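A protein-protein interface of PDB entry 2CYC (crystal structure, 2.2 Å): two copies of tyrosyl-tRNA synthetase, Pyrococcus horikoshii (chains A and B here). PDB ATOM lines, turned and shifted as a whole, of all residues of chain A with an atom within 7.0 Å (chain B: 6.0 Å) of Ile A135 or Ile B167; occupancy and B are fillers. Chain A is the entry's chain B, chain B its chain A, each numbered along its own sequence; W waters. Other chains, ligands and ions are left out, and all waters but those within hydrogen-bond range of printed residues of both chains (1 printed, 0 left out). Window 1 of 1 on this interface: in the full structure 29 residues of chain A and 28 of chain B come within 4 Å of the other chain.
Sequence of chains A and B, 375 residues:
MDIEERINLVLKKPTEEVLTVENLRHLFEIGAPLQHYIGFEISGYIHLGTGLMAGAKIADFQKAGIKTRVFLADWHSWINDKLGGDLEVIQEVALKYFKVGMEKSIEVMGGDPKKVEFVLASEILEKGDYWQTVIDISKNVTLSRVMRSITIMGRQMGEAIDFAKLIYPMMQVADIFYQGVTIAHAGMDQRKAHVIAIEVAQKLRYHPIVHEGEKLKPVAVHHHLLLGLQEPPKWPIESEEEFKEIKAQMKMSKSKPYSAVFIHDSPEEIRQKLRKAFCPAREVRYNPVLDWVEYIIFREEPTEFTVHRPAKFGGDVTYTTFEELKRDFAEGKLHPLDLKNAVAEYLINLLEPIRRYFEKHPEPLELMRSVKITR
O of Trp B78 is in hydrogen-bond range of NZ of Lys A139 (3.2 Å).
O of Ser A138 is in hydrogen-bond range of N of Phe B163.
The backbone NH of Ala B164 sits at hydrogen-bond distance from the backbone carbonyl oxygen of Ser A138 (3.2 Å).
CG of Trp B131 touches CG of Trp A131 (3.2 Å).
Ile A135 touches Trp B78 (CG2 to CZ3, 3.5 Å).
O of Ile A135 touches CB of Ala B164, at 3.97 Å.
Ile B167 touches Ile A135 (CD1 to CD1, 3.9 Å).
Trp B78 touches Asp A136.
Ala B164 touches Lys A139 (CB to CG, 3.6 Å).
Met B170 touches Phe A163.
CZ of Phe B163 touches N of Ile A167 (3.9 Å).
Met A170 touches Phe B163.
Tyr A206 touches Trp B78.
Water W1 bridges the side-chain carboxylate (OD1) of Asp A136 (2.7 Å) and the indole nitrogen (NE1) of Trp B78 (3.3 Å).
Of the printed residues of chain B, Ile A135 touches Trp B78 (3.5 Å), Ile B79 (3.5 Å), Trp B131 (3.998 Å), Ala B164 (3.97 Å) and Ile B167 (3.9 Å).
Of the printed residues of chain B, Lys A139 touches Trp B78 (3.2 Å), Ile B79 (3.6 Å) and Ala B164 (3.6 Å).
Of the printed residues of chain A, Trp B78 touches Gln A132, Ile A135, Asp A136, Lys A139 and Tyr A206.
Lys B165 touches none of the printed residues of chain A.
Ile B167 touches three residues of chain A.
Pro B169 touches none of the printed residues of chain A.
The backbone carbonyl oxygen of Ile B79 is in hydrogen-bond range of the side-chain amino group of Lys B165, 3.1 Å away.
The backbone carbonyl oxygen (O) of Asp A136 lies close to the side-chain amide oxygen (OD1) of Asn A140, at 2.9 Å.
O of Val A134 lies within hydrogen-bond range of OG of Ser A138, 2.7 Å away.
Hydrophobic or aromatic side chains of chain B that line the printed part of chain A: Trp B75, Trp B78, Ile B79, Trp B131, Val B146, Phe B163, Ala B164, Leu B166, Ile B167 and Met B170.
Printed residues of chain A that touch a printed residue of chain B: Trp A131, Gln A132, Ile A135, Asp A136, Ser A138, Lys A139, Phe A163, Ile A167, Met A170 and Tyr A206.
Hydrophobic or aromatic side chains of chain A that line the printed part of chain B: Trp A131, Ile A135, Phe A163, Met A170 and Tyr A206.
Among the printed residues, 23 pairs touch across the chains.
Trp A131 touches its own counterpart, Trp B131.
Phe A163 touches its own counterpart, Phe B163.
Phe A163 touches Ile B167, and with the chains exchanged Ile A167 touches Phe B163.
Phe A163 touches Met B170, and with the chains exchanged Met A170 touches Phe B163.
5 positions are printed for both chains.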
ATOM      1  N   TYR A 130      17.948  -5.923  12.973  1.00  0.00           N
ATOM      2  CA  TYR A 130      18.897  -6.937  13.397  1.00  0.00           C
ATOM      3  C   TYR A 130      19.288  -7.694  12.137  1.00  0.00           C
ATOM      4  O   TYR A 130      20.471  -7.919  11.859  1.00  0.00           O
ATOM      5  CB  TYR A 130      18.255  -7.917  14.373  1.00  0.00           C
ATOM      6  CG  TYR A 130      19.039  -9.204  14.517  1.00  0.00           C
ATOM      7  CD1 TYR A 130      20.094  -9.312  15.435  1.00  0.00           C
ATOM      8  CD2 TYR A 130      18.741 -10.314  13.721  1.00  0.00           C
ATOM      9  CE1 TYR A 130      20.832 -10.512  15.561  1.00  0.00           C
ATOM     10  CE2 TYR A 130      19.465 -11.500  13.830  1.00  0.00           C
ATOM     11  CZ  TYR A 130      20.505 -11.599  14.753  1.00  0.00           C
ATOM     12  OH  TYR A 130      21.177 -12.797  14.877  1.00  0.00           O
ATOM     13  N   TRP A 131      18.283  -8.073  11.356  1.00  0.00           N
ATOM     14  CA  TRP A 131      18.549  -8.821  10.137  1.00  0.00           C
ATOM     15  C   TRP A 131      19.307  -8.026   9.085  1.00  0.00           C
ATOM     16  O   TRP A 131      20.055  -8.590   8.275  1.00  0.00           O
ATOM     17  CB  TRP A 131      17.245  -9.408   9.595  1.00  0.00           C
ATOM     18  CG  TRP A 131      16.784 -10.496  10.512  1.00  0.00           C
ATOM     19  CD1 TRP A 131      15.933 -10.371  11.570  1.00  0.00           C
ATOM     20  CD2 TRP A 131      17.286 -11.838  10.557  1.00  0.00           C
ATOM     21  NE1 TRP A 131      15.880 -11.551  12.280  1.00  0.00           N
ATOM     22  CE2 TRP A 131      16.704 -12.466  11.678  1.00  0.00           C
ATOM     23  CE3 TRP A 131      18.179 -12.566   9.761  1.00  0.00           C
ATOM     24  CZ2 TRP A 131      16.988 -13.793  12.026  1.00  0.00           C
ATOM     25  CZ3 TRP A 131      18.463 -13.894  10.112  1.00  0.00           C
ATOM     26  CH2 TRP A 131      17.867 -14.487  11.232  1.00  0.00           C
ATOM     27  N   GLN A 132      19.137  -6.713   9.102  1.00  0.00           N
ATOM     28  CA  GLN A 132      19.870  -5.890   8.162  1.00  0.00           C
ATOM     29  C   GLN A 132      21.352  -6.048   8.505  1.00  0.00           C
ATOM     30  O   GLN A 132      22.221  -6.039   7.627  1.00  0.00           O
ATOM     31  CB  GLN A 132      19.445  -4.427   8.285  1.00  0.00           C
ATOM     32  CG  GLN A 132      20.186  -3.511   7.321  1.00  0.00           C
ATOM     33  CD  GLN A 132      19.579  -2.120   7.252  1.00  0.00           C
ATOM     34  OE1 GLN A 132      19.232  -1.533   8.274  1.00  0.00           O
ATOM     35  NE2 GLN A 132      19.464  -1.583   6.044  1.00  0.00           N
ATOM     36  N   THR A 133      21.644  -6.202   9.790  1.00  0.00           N
ATOM     37  CA  THR A 133      23.031  -6.367  10.197  1.00  0.00           C
ATOM     38  C   THR A 133      23.513  -7.778   9.859  1.00  0.00           C
ATOM     39  O   THR A 133      24.678  -7.981   9.556  1.00  0.00           O
ATOM     40  CB  THR A 133      23.206  -5.993  11.687  1.00  0.00           C
ATOM     41  OG1 THR A 133      23.514  -4.592  11.761  1.00  0.00           O
ATOM     42  CG2 THR A 133      24.323  -6.802  12.358  1.00  0.00           C
ATOM     43  N   VAL A 134      22.615  -8.753   9.877  1.00  0.00           N
ATOM     44  CA  VAL A 134      23.014 -10.105   9.489  1.00  0.00           C
ATOM     45  C   VAL A 134      23.467 -10.033   8.033  1.00  0.00           C
ATOM     46  O   VAL A 134      24.458 -10.655   7.653  1.00  0.00           O
ATOM     47  CB  VAL A 134      21.842 -11.111   9.579  1.00  0.00           C
ATOM     48  CG1 VAL A 134      22.234 -12.433   8.924  1.00  0.00           C
ATOM     49  CG2 VAL A 134      21.477 -11.343  11.036  1.00  0.00           C
ATOM     50  N   ILE A 135      22.734  -9.278   7.218  1.00  0.00           N
ATOM     51  CA  ILE A 135      23.074  -9.144   5.801  1.00  0.00           C
ATOM     52  C   ILE A 135      24.399  -8.390   5.669  1.00  0.00           C
ATOM     53  O   ILE A 135      25.288  -8.800   4.917  1.00  0.00           O
ATOM     54  CB  ILE A 135      21.976  -8.370   5.016  1.00  0.00           C
ATOM     55  CG1 ILE A 135      20.662  -9.156   5.022  1.00  0.00           C
ATOM     56  CG2 ILE A 135      22.420  -8.145   3.583  1.00  0.00           C
ATOM     57  CD1 ILE A 135      20.777 -10.553   4.420  1.00  0.00           C
ATOM     58  N   ASP A 136      24.522  -7.293   6.408  1.00  0.00           N
ATOM     59  CA  ASP A 136      25.733  -6.472   6.395  1.00  0.00           C
ATOM     60  C   ASP A 136      26.948  -7.355   6.697  1.00  0.00           C
ATOM     61  O   ASP A 136      27.934  -7.327   5.966  1.00  0.00           O
ATOM     62  CB  ASP A 136      25.611  -5.327   7.426  1.00  0.00           C
ATOM     63  CG  ASP A 136      26.755  -4.303   7.324  1.00  0.00           C
ATOM     64  OD1 ASP A 136      27.237  -4.032   6.197  1.00  0.00           O
ATOM     65  OD2 ASP A 136      27.159  -3.756   8.369  1.00  0.00           O
ATOM     66  N   ILE A 137      26.865  -8.151   7.758  1.00  0.00           N
ATOM     67  CA  ILE A 137      27.961  -9.061   8.112  1.00  0.00           C
ATOM     68  C   ILE A 137      28.188 -10.091   6.997  1.00  0.00           C
ATOM     69  O   ILE A 137      29.321 -10.331   6.572  1.00  0.00           O
ATOM     70  CB  ILE A 137      27.651  -9.819   9.427  1.00  0.00           C
ATOM     71  CG1 ILE A 137      27.653  -8.839  10.599  1.00  0.00           C
ATOM     72  CG2 ILE A 137      28.662 -10.962   9.646  1.00  0.00           C
ATOM     73  CD1 ILE A 137      27.034  -9.414  11.886  1.00  0.00           C
ATOM     74  N   SER A 138      27.105 -10.688   6.513  1.00  0.00           N
ATOM     75  CA  SER A 138      27.201 -11.705   5.466  1.00  0.00           C
ATOM     76  C   SER A 138      27.854 -11.231   4.164  1.00  0.00           C
ATOM     77  O   SER A 138      28.421 -12.041   3.425  1.00  0.00           O
ATOM     78  CB  SER A 138      25.818 -12.276   5.171  1.00  0.00           C
ATOM     79  OG  SER A 138      25.278 -12.895   6.324  1.00  0.00           O
ATOM     80  N   LYS A 139      27.763  -9.937   3.870  1.00  0.00           N
ATOM     81  CA  LYS A 139      28.381  -9.399   2.657  1.00  0.00           C
ATOM     82  C   LYS A 139      29.896  -9.381   2.834  1.00  0.00           C
ATOM     83  O   LYS A 139      30.631  -9.191   1.869  1.00  0.00           O
ATOM     84  CB  LYS A 139      27.908  -7.964   2.374  1.00  0.00           C
ATOM     85  CG  LYS A 139      26.490  -7.839   1.832  1.00  0.00           C
ATOM     86  CD  LYS A 139      26.088  -6.369   1.577  1.00  0.00           C
ATOM     87  CE  LYS A 139      26.963  -5.672   0.527  1.00  0.00           C
ATOM     88  NZ  LYS A 139      26.867  -6.286  -0.831  1.00  0.00           N
ATOM     89  N   ASN A 140      30.354  -9.572   4.070  1.00  0.00           N
ATOM     90  CA  ASN A 140      31.781  -9.552   4.365  1.00  0.00           C
ATOM     91  C   ASN A 140      32.382 -10.910   4.664  1.00  0.00           C
ATOM     92  O   ASN A 140      33.554 -11.003   5.003  1.00  0.00           O
ATOM     93  CB  ASN A 140      32.068  -8.606   5.534  1.00  0.00           C
ATOM     94  CG  ASN A 140      31.772  -7.157   5.190  1.00  0.00           C
ATOM     95  OD1 ASN A 140      30.730  -6.614   5.558  1.00  0.00           O
ATOM     96  ND2 ASN A 140      32.687  -6.528   4.464  1.00  0.00           N
ATOM     97  N   PHE A 163      19.800 -25.167   4.306  1.00  0.00           N
ATOM     98  CA  PHE A 163      20.405 -23.837   4.259  1.00  0.00           C
ATOM     99  C   PHE A 163      20.315 -23.047   5.559  1.00  0.00           C
ATOM    100  O   PHE A 163      21.210 -22.254   5.866  1.00  0.00           O
ATOM    101  CB  PHE A 163      19.791 -23.017   3.106  1.00  0.00           C
ATOM    102  CG  PHE A 163      20.452 -21.683   2.891  1.00  0.00           C
ATOM    103  CD1 PHE A 163      19.806 -20.499   3.265  1.00  0.00           C
ATOM    104  CD2 PHE A 163      21.749 -21.611   2.364  1.00  0.00           C
ATOM    105  CE1 PHE A 163      20.445 -19.255   3.123  1.00  0.00           C
ATOM    106  CE2 PHE A 163      22.402 -20.377   2.215  1.00  0.00           C
ATOM    107  CZ  PHE A 163      21.747 -19.191   2.597  1.00  0.00           C
ATOM    108  N   ILE A 167      22.888 -20.103   7.946  1.00  0.00           N
ATOM    109  CA  ILE A 167      22.568 -18.745   8.402  1.00  0.00           C
ATOM    110  C   ILE A 167      22.939 -18.586   9.882  1.00  0.00           C
ATOM    111  O   ILE A 167      23.318 -17.502  10.337  1.00  0.00           O
ATOM    112  CB  ILE A 167      21.065 -18.447   8.223  1.00  0.00           C
ATOM    113  CG1 ILE A 167      20.692 -18.586   6.742  1.00  0.00           C
ATOM    114  CG2 ILE A 167      20.742 -17.031   8.718  1.00  0.00           C
ATOM    115  CD1 ILE A 167      19.204 -18.513   6.477  1.00  0.00           C
ATOM    116  N   MET A 170      26.108 -16.725  11.024  1.00  0.00           N
ATOM    117  CA  MET A 170      26.026 -15.295  10.763  1.00  0.00           C
ATOM    118  C   MET A 170      25.137 -14.643  11.815  1.00  0.00           C
ATOM    119  O   MET A 170      25.331 -13.484  12.176  1.00  0.00           O
ATOM    120  CB  MET A 170      25.505 -15.041   9.347  1.00  0.00           C
ATOM    121  CG  MET A 170      26.471 -15.530   8.274  1.00  0.00           C
ATOM    122  SD  MET A 170      28.090 -14.699   8.298  1.00  0.00           S
ATOM    123  CE  MET A 170      29.028 -15.716   9.520  1.00  0.00           C
ATOM    124  N   ALA A 174      26.123 -11.632  14.335  1.00  0.00           N
ATOM    125  CA  ALA A 174      25.216 -10.491  14.440  1.00  0.00           C
ATOM    126  C   ALA A 174      24.768 -10.279  15.887  1.00  0.00           C
ATOM    127  O   ALA A 174      24.593  -9.143  16.329  1.00  0.00           O
ATOM    128  CB  ALA A 174      23.984 -10.703  13.530  1.00  0.00           C
ATOM    129  N   TYR A 206      25.902  -0.834  10.099  1.00  0.00           N
ATOM    130  CA  TYR A 206      24.796  -0.566  11.005  1.00  0.00           C
ATOM    131  C   TYR A 206      25.033  -0.778  12.483  1.00  0.00           C
ATOM    132  O   TYR A 206      24.559   0.007  13.302  1.00  0.00           O
ATOM    133  CB  TYR A 206      23.563  -1.351  10.545  1.00  0.00           C
ATOM    134  CG  TYR A 206      23.261  -1.091   9.090  1.00  0.00           C
ATOM    135  CD1 TYR A 206      23.660  -1.988   8.107  1.00  0.00           C
ATOM    136  CD2 TYR A 206      22.639   0.096   8.687  1.00  0.00           C
ATOM    137  CE1 TYR A 206      23.451  -1.718   6.754  1.00  0.00           C
ATOM    138  CE2 TYR A 206      22.433   0.380   7.336  1.00  0.00           C
ATOM    139  CZ  TYR A 206      22.840  -0.531   6.377  1.00  0.00           C
ATOM    140  OH  TYR A 206      22.640  -0.263   5.040  1.00  0.00           O
ATOM    141  N   TRP B  75      16.927  -4.129  -0.757  1.00  0.00           N
ATOM    142  CA  TRP B  75      17.987  -4.861  -0.052  1.00  0.00           C
ATOM    143  C   TRP B  75      18.580  -5.919  -0.972  1.00  0.00           C
ATOM    144  O   TRP B  75      19.787  -6.182  -0.932  1.00  0.00           O
ATOM    145  CB  TRP B  75      17.464  -5.547   1.219  1.00  0.00           C
ATOM    146  CG  TRP B  75      17.195  -4.620   2.360  1.00  0.00           C
ATOM    147  CD1 TRP B  75      16.942  -3.273   2.286  1.00  0.00           C
ATOM    148  CD2 TRP B  75      17.045  -4.980   3.740  1.00  0.00           C
ATOM    149  NE1 TRP B  75      16.638  -2.780   3.535  1.00  0.00           N
ATOM    150  CE2 TRP B  75      16.692  -3.803   4.446  1.00  0.00           C
ATOM    151  CE3 TRP B  75      17.167  -6.185   4.450  1.00  0.00           C
ATOM    152  CZ2 TRP B  75      16.459  -3.794   5.831  1.00  0.00           C
ATOM    153  CZ3 TRP B  75      16.934  -6.180   5.832  1.00  0.00           C
ATOM    154  CH2 TRP B  75      16.584  -4.988   6.504  1.00  0.00           C
ATOM    155  N   TRP B  78      21.026  -4.334  -3.109  1.00  0.00           N
ATOM    156  CA  TRP B  78      22.162  -3.962  -2.272  1.00  0.00           C
ATOM    157  C   TRP B  78      23.060  -5.201  -2.127  1.00  0.00           C
ATOM    158  O   TRP B  78      24.281  -5.134  -2.293  1.00  0.00           O
ATOM    159  CB  TRP B  78      21.627  -3.486  -0.915  1.00  0.00           C
ATOM    160  CG  TRP B  78      22.598  -3.505   0.239  1.00  0.00           C
ATOM    161  CD1 TRP B  78      23.901  -3.080   0.235  1.00  0.00           C
ATOM    162  CD2 TRP B  78      22.319  -3.941   1.577  1.00  0.00           C
ATOM    163  NE1 TRP B  78      24.448  -3.224   1.494  1.00  0.00           N
ATOM    164  CE2 TRP B  78      23.501  -3.751   2.336  1.00  0.00           C
ATOM    165  CE3 TRP B  78      21.178  -4.473   2.213  1.00  0.00           C
ATOM    166  CZ2 TRP B  78      23.583  -4.079   3.703  1.00  0.00           C
ATOM    167  CZ3 TRP B  78      21.254  -4.798   3.570  1.00  0.00           C
ATOM    168  CH2 TRP B  78      22.456  -4.599   4.303  1.00  0.00           C
ATOM    169  N   ILE B  79      22.432  -6.335  -1.838  1.00  0.00           N
ATOM    170  CA  ILE B  79      23.136  -7.604  -1.692  1.00  0.00           C
ATOM    171  C   ILE B  79      23.822  -7.977  -2.999  1.00  0.00           C
ATOM    172  O   ILE B  79      24.959  -8.463  -3.010  1.00  0.00           O
ATOM    173  CB  ILE B  79      22.149  -8.733  -1.326  1.00  0.00           C
ATOM    174  CG1 ILE B  79      21.749  -8.611   0.146  1.00  0.00           C
ATOM    175  CG2 ILE B  79      22.757 -10.096  -1.652  1.00  0.00           C
ATOM    176  CD1 ILE B  79      20.674  -9.610   0.561  1.00  0.00           C
ATOM    177  N   TRP B 131      11.658 -12.372   8.544  1.00  0.00           N
ATOM    178  CA  TRP B 131      12.887 -13.160   8.617  1.00  0.00           C
ATOM    179  C   TRP B 131      12.689 -14.515   9.279  1.00  0.00           C
ATOM    180  O   TRP B 131      13.423 -15.477   8.998  1.00  0.00           O
ATOM    181  CB  TRP B 131      13.988 -12.346   9.304  1.00  0.00           C
ATOM    182  CG  TRP B 131      14.428 -11.221   8.405  1.00  0.00           C
ATOM    183  CD1 TRP B 131      13.931  -9.944   8.372  1.00  0.00           C
ATOM    184  CD2 TRP B 131      15.315 -11.330   7.288  1.00  0.00           C
ATOM    185  NE1 TRP B 131      14.448  -9.258   7.292  1.00  0.00           N
ATOM    186  CE2 TRP B 131      15.298 -10.089   6.611  1.00  0.00           C
ATOM    187  CE3 TRP B 131      16.115 -12.359   6.789  1.00  0.00           C
ATOM    188  CZ2 TRP B 131      16.056  -9.854   5.459  1.00  0.00           C
ATOM    189  CZ3 TRP B 131      16.870 -12.124   5.638  1.00  0.00           C
ATOM    190  CH2 TRP B 131      16.834 -10.884   4.990  1.00  0.00           C
ATOM    191  N   VAL B 134      11.953 -16.475   6.517  1.00  0.00           N
ATOM    192  CA  VAL B 134      13.113 -16.755   5.673  1.00  0.00           C
ATOM    193  C   VAL B 134      13.763 -18.018   6.268  1.00  0.00           C
ATOM    194  O   VAL B 134      14.167 -18.933   5.539  1.00  0.00           O
ATOM    195  CB  VAL B 134      14.156 -15.608   5.693  1.00  0.00           C
ATOM    196  CG1 VAL B 134      15.475 -16.110   5.114  1.00  0.00           C
ATOM    197  CG2 VAL B 134      13.651 -14.404   4.864  1.00  0.00           C
ATOM    198  N   VAL B 146      20.144 -24.087  -2.920  1.00  0.00           N
ATOM    199  CA  VAL B 146      20.260 -22.635  -2.959  1.00  0.00           C
ATOM    200  C   VAL B 146      21.398 -22.235  -3.894  1.00  0.00           C
ATOM    201  O   VAL B 146      21.268 -21.296  -4.678  1.00  0.00           O
ATOM    202  CB  VAL B 146      20.554 -22.038  -1.563  1.00  0.00           C
ATOM    203  CG1 VAL B 146      20.731 -20.516  -1.680  1.00  0.00           C
ATOM    204  CG2 VAL B 146      19.419 -22.388  -0.594  1.00  0.00           C
ATOM    205  N   PHE B 163      28.541 -14.636   1.495  1.00  0.00           N
ATOM    206  CA  PHE B 163      27.381 -15.360   1.972  1.00  0.00           C
ATOM    207  C   PHE B 163      26.032 -14.689   1.753  1.00  0.00           C
ATOM    208  O   PHE B 163      25.030 -15.378   1.539  1.00  0.00           O
ATOM    209  CB  PHE B 163      27.541 -15.719   3.455  1.00  0.00           C
ATOM    210  CG  PHE B 163      26.464 -16.644   3.961  1.00  0.00           C
ATOM    211  CD1 PHE B 163      25.486 -16.186   4.834  1.00  0.00           C
ATOM    212  CD2 PHE B 163      26.397 -17.961   3.508  1.00  0.00           C
ATOM    213  CE1 PHE B 163      24.445 -17.025   5.249  1.00  0.00           C
ATOM    214  CE2 PHE B 163      25.362 -18.812   3.914  1.00  0.00           C
ATOM    215  CZ  PHE B 163      24.379 -18.340   4.788  1.00  0.00           C
ATOM    216  N   ALA B 164      25.999 -13.360   1.798  1.00  0.00           N
ATOM    217  CA  ALA B 164      24.747 -12.628   1.626  1.00  0.00           C
ATOM    218  C   ALA B 164      24.041 -12.977   0.323  1.00  0.00           C
ATOM    219  O   ALA B 164      22.812 -13.010   0.280  1.00  0.00           O
ATOM    220  CB  ALA B 164      24.991 -11.109   1.696  1.00  0.00           C
ATOM    221  N   LYS B 165      24.815 -13.239  -0.733  1.00  0.00           N
ATOM    222  CA  LYS B 165      24.232 -13.575  -2.032  1.00  0.00           C
ATOM    223  C   LYS B 165      23.472 -14.885  -2.017  1.00  0.00           C
ATOM    224  O   LYS B 165      22.548 -15.075  -2.810  1.00  0.00           O
ATOM    225  CB  LYS B 165      25.307 -13.597  -3.123  1.00  0.00           C
ATOM    226  CG  LYS B 165      25.808 -12.196  -3.472  1.00  0.00           C
ATOM    227  CD  LYS B 165      26.828 -12.201  -4.609  1.00  0.00           C
ATOM    228  CE  LYS B 165      27.105 -10.783  -5.086  1.00  0.00           C
ATOM    229  NZ  LYS B 165      27.503  -9.891  -3.963  1.00  0.00           N
ATOM    230  N   LEU B 166      23.858 -15.785  -1.115  1.00  0.00           N
ATOM    231  CA  LEU B 166      23.173 -17.072  -0.972  1.00  0.00           C
ATOM    232  C   LEU B 166      21.860 -16.861  -0.205  1.00  0.00           C
ATOM    233  O   LEU B 166      20.925 -17.647  -0.328  1.00  0.00           O
ATOM    234  CB  LEU B 166      24.054 -18.076  -0.218  1.00  0.00           C
ATOM    235  CG  LEU B 166      25.100 -18.860  -1.026  1.00  0.00           C
ATOM    236  CD1 LEU B 166      24.383 -19.767  -2.004  1.00  0.00           C
ATOM    237  CD2 LEU B 166      26.030 -17.915  -1.768  1.00  0.00           C
ATOM    238  N   ILE B 167      21.792 -15.804   0.598  1.00  0.00           N
ATOM    239  CA  ILE B 167      20.561 -15.532   1.339  1.00  0.00           C
ATOM    240  C   ILE B 167      19.486 -14.993   0.381  1.00  0.00           C
ATOM    241  O   ILE B 167      18.298 -15.293   0.516  1.00  0.00           O
ATOM    242  CB  ILE B 167      20.820 -14.507   2.472  1.00  0.00           C
ATOM    243  CG1 ILE B 167      21.836 -15.089   3.466  1.00  0.00           C
ATOM    244  CG2 ILE B 167      19.500 -14.149   3.179  1.00  0.00           C
ATOM    245  CD1 ILE B 167      22.278 -14.106   4.531  1.00  0.00           C
ATOM    246  N   TYR B 168      19.922 -14.207  -0.599  1.00  0.00           N
ATOM    247  CA  TYR B 168      19.037 -13.600  -1.604  1.00  0.00           C
ATOM    248  C   TYR B 168      17.919 -14.520  -2.150  1.00  0.00           C
ATOM    249  O   TYR B 168      16.741 -14.158  -2.141  1.00  0.00           O
ATOM    250  CB  TYR B 168      19.916 -13.061  -2.755  1.00  0.00           C
ATOM    251  CG  TYR B 168      19.219 -12.333  -3.901  1.00  0.00           C
ATOM    252  CD1 TYR B 168      19.665 -11.081  -4.312  1.00  0.00           C
ATOM    253  CD2 TYR B 168      18.187 -12.930  -4.631  1.00  0.00           C
ATOM    254  CE1 TYR B 168      19.118 -10.438  -5.417  1.00  0.00           C
ATOM    255  CE2 TYR B 168      17.630 -12.294  -5.745  1.00  0.00           C
ATOM    256  CZ  TYR B 168      18.104 -11.046  -6.130  1.00  0.00           C
ATOM    257  OH  TYR B 168      17.566 -10.397  -7.223  1.00  0.00           O
ATOM    258  N   PRO B 169      18.261 -15.725  -2.615  1.00  0.00           N
ATOM    259  CA  PRO B 169      17.177 -16.572  -3.136  1.00  0.00           C
ATOM    260  C   PRO B 169      16.124 -16.959  -2.089  1.00  0.00           C
ATOM    261  O   PRO B 169      14.947 -17.114  -2.406  1.00  0.00           O
ATOM    262  CB  PRO B 169      17.923 -17.788  -3.694  1.00  0.00           C
ATOM    263  CG  PRO B 169      19.308 -17.227  -4.019  1.00  0.00           C
ATOM    264  CD  PRO B 169      19.569 -16.371  -2.805  1.00  0.00           C
ATOM    265  N   MET B 170      16.549 -17.135  -0.844  1.00  0.00           N
ATOM    266  CA  MET B 170      15.608 -17.496   0.200  1.00  0.00           C
ATOM    267  C   MET B 170      14.720 -16.290   0.519  1.00  0.00           C
ATOM    268  O   MET B 170      13.568 -16.437   0.927  1.00  0.00           O
ATOM    269  CB  MET B 170      16.367 -17.992   1.441  1.00  0.00           C
ATOM    270  CG  MET B 170      17.131 -19.294   1.179  1.00  0.00           C
ATOM    271  SD  MET B 170      16.060 -20.693   0.711  1.00  0.00           S
ATOM    272  CE  MET B 170      16.042 -20.562  -1.113  1.00  0.00           C
ATOM    273  N   MET B 171      15.258 -15.094   0.317  1.00  0.00           N
ATOM    274  CA  MET B 171      14.484 -13.880   0.542  1.00  0.00           C
ATOM    275  C   MET B 171      13.422 -13.755  -0.558  1.00  0.00           C
ATOM    276  O   MET B 171      12.297 -13.325  -0.296  1.00  0.00           O
ATOM    277  CB  MET B 171      15.398 -12.649   0.514  1.00  0.00           C
ATOM    278  CG  MET B 171      16.275 -12.476   1.745  1.00  0.00           C
ATOM    279  SD  MET B 171      17.561 -11.232   1.456  1.00  0.00           S
ATOM    280  CE  MET B 171      16.539  -9.736   1.215  1.00  0.00           C
ATOM    281  N   GLN B 172      13.777 -14.136  -1.786  1.00  0.00           N
ATOM    282  CA  GLN B 172      12.834 -14.044  -2.900  1.00  0.00           C
ATOM    283  C   GLN B 172      11.664 -14.984  -2.658  1.00  0.00           C
ATOM    284  O   GLN B 172      10.509 -14.626  -2.920  1.00  0.00           O
ATOM    285  CB  GLN B 172      13.504 -14.381  -4.247  1.00  0.00           C
ATOM    286  CG  GLN B 172      12.568 -14.186  -5.476  1.00  0.00           C
ATOM    287  CD  GLN B 172      13.321 -13.936  -6.780  1.00  0.00           C
ATOM    288  OE1 GLN B 172      14.481 -13.530  -6.759  1.00  0.00           O
ATOM    289  NE2 GLN B 172      12.652 -14.149  -7.922  1.00  0.00           N
HETATM  290  O   HOH W   1      26.903  -2.997   3.753  1.00  0.00           O
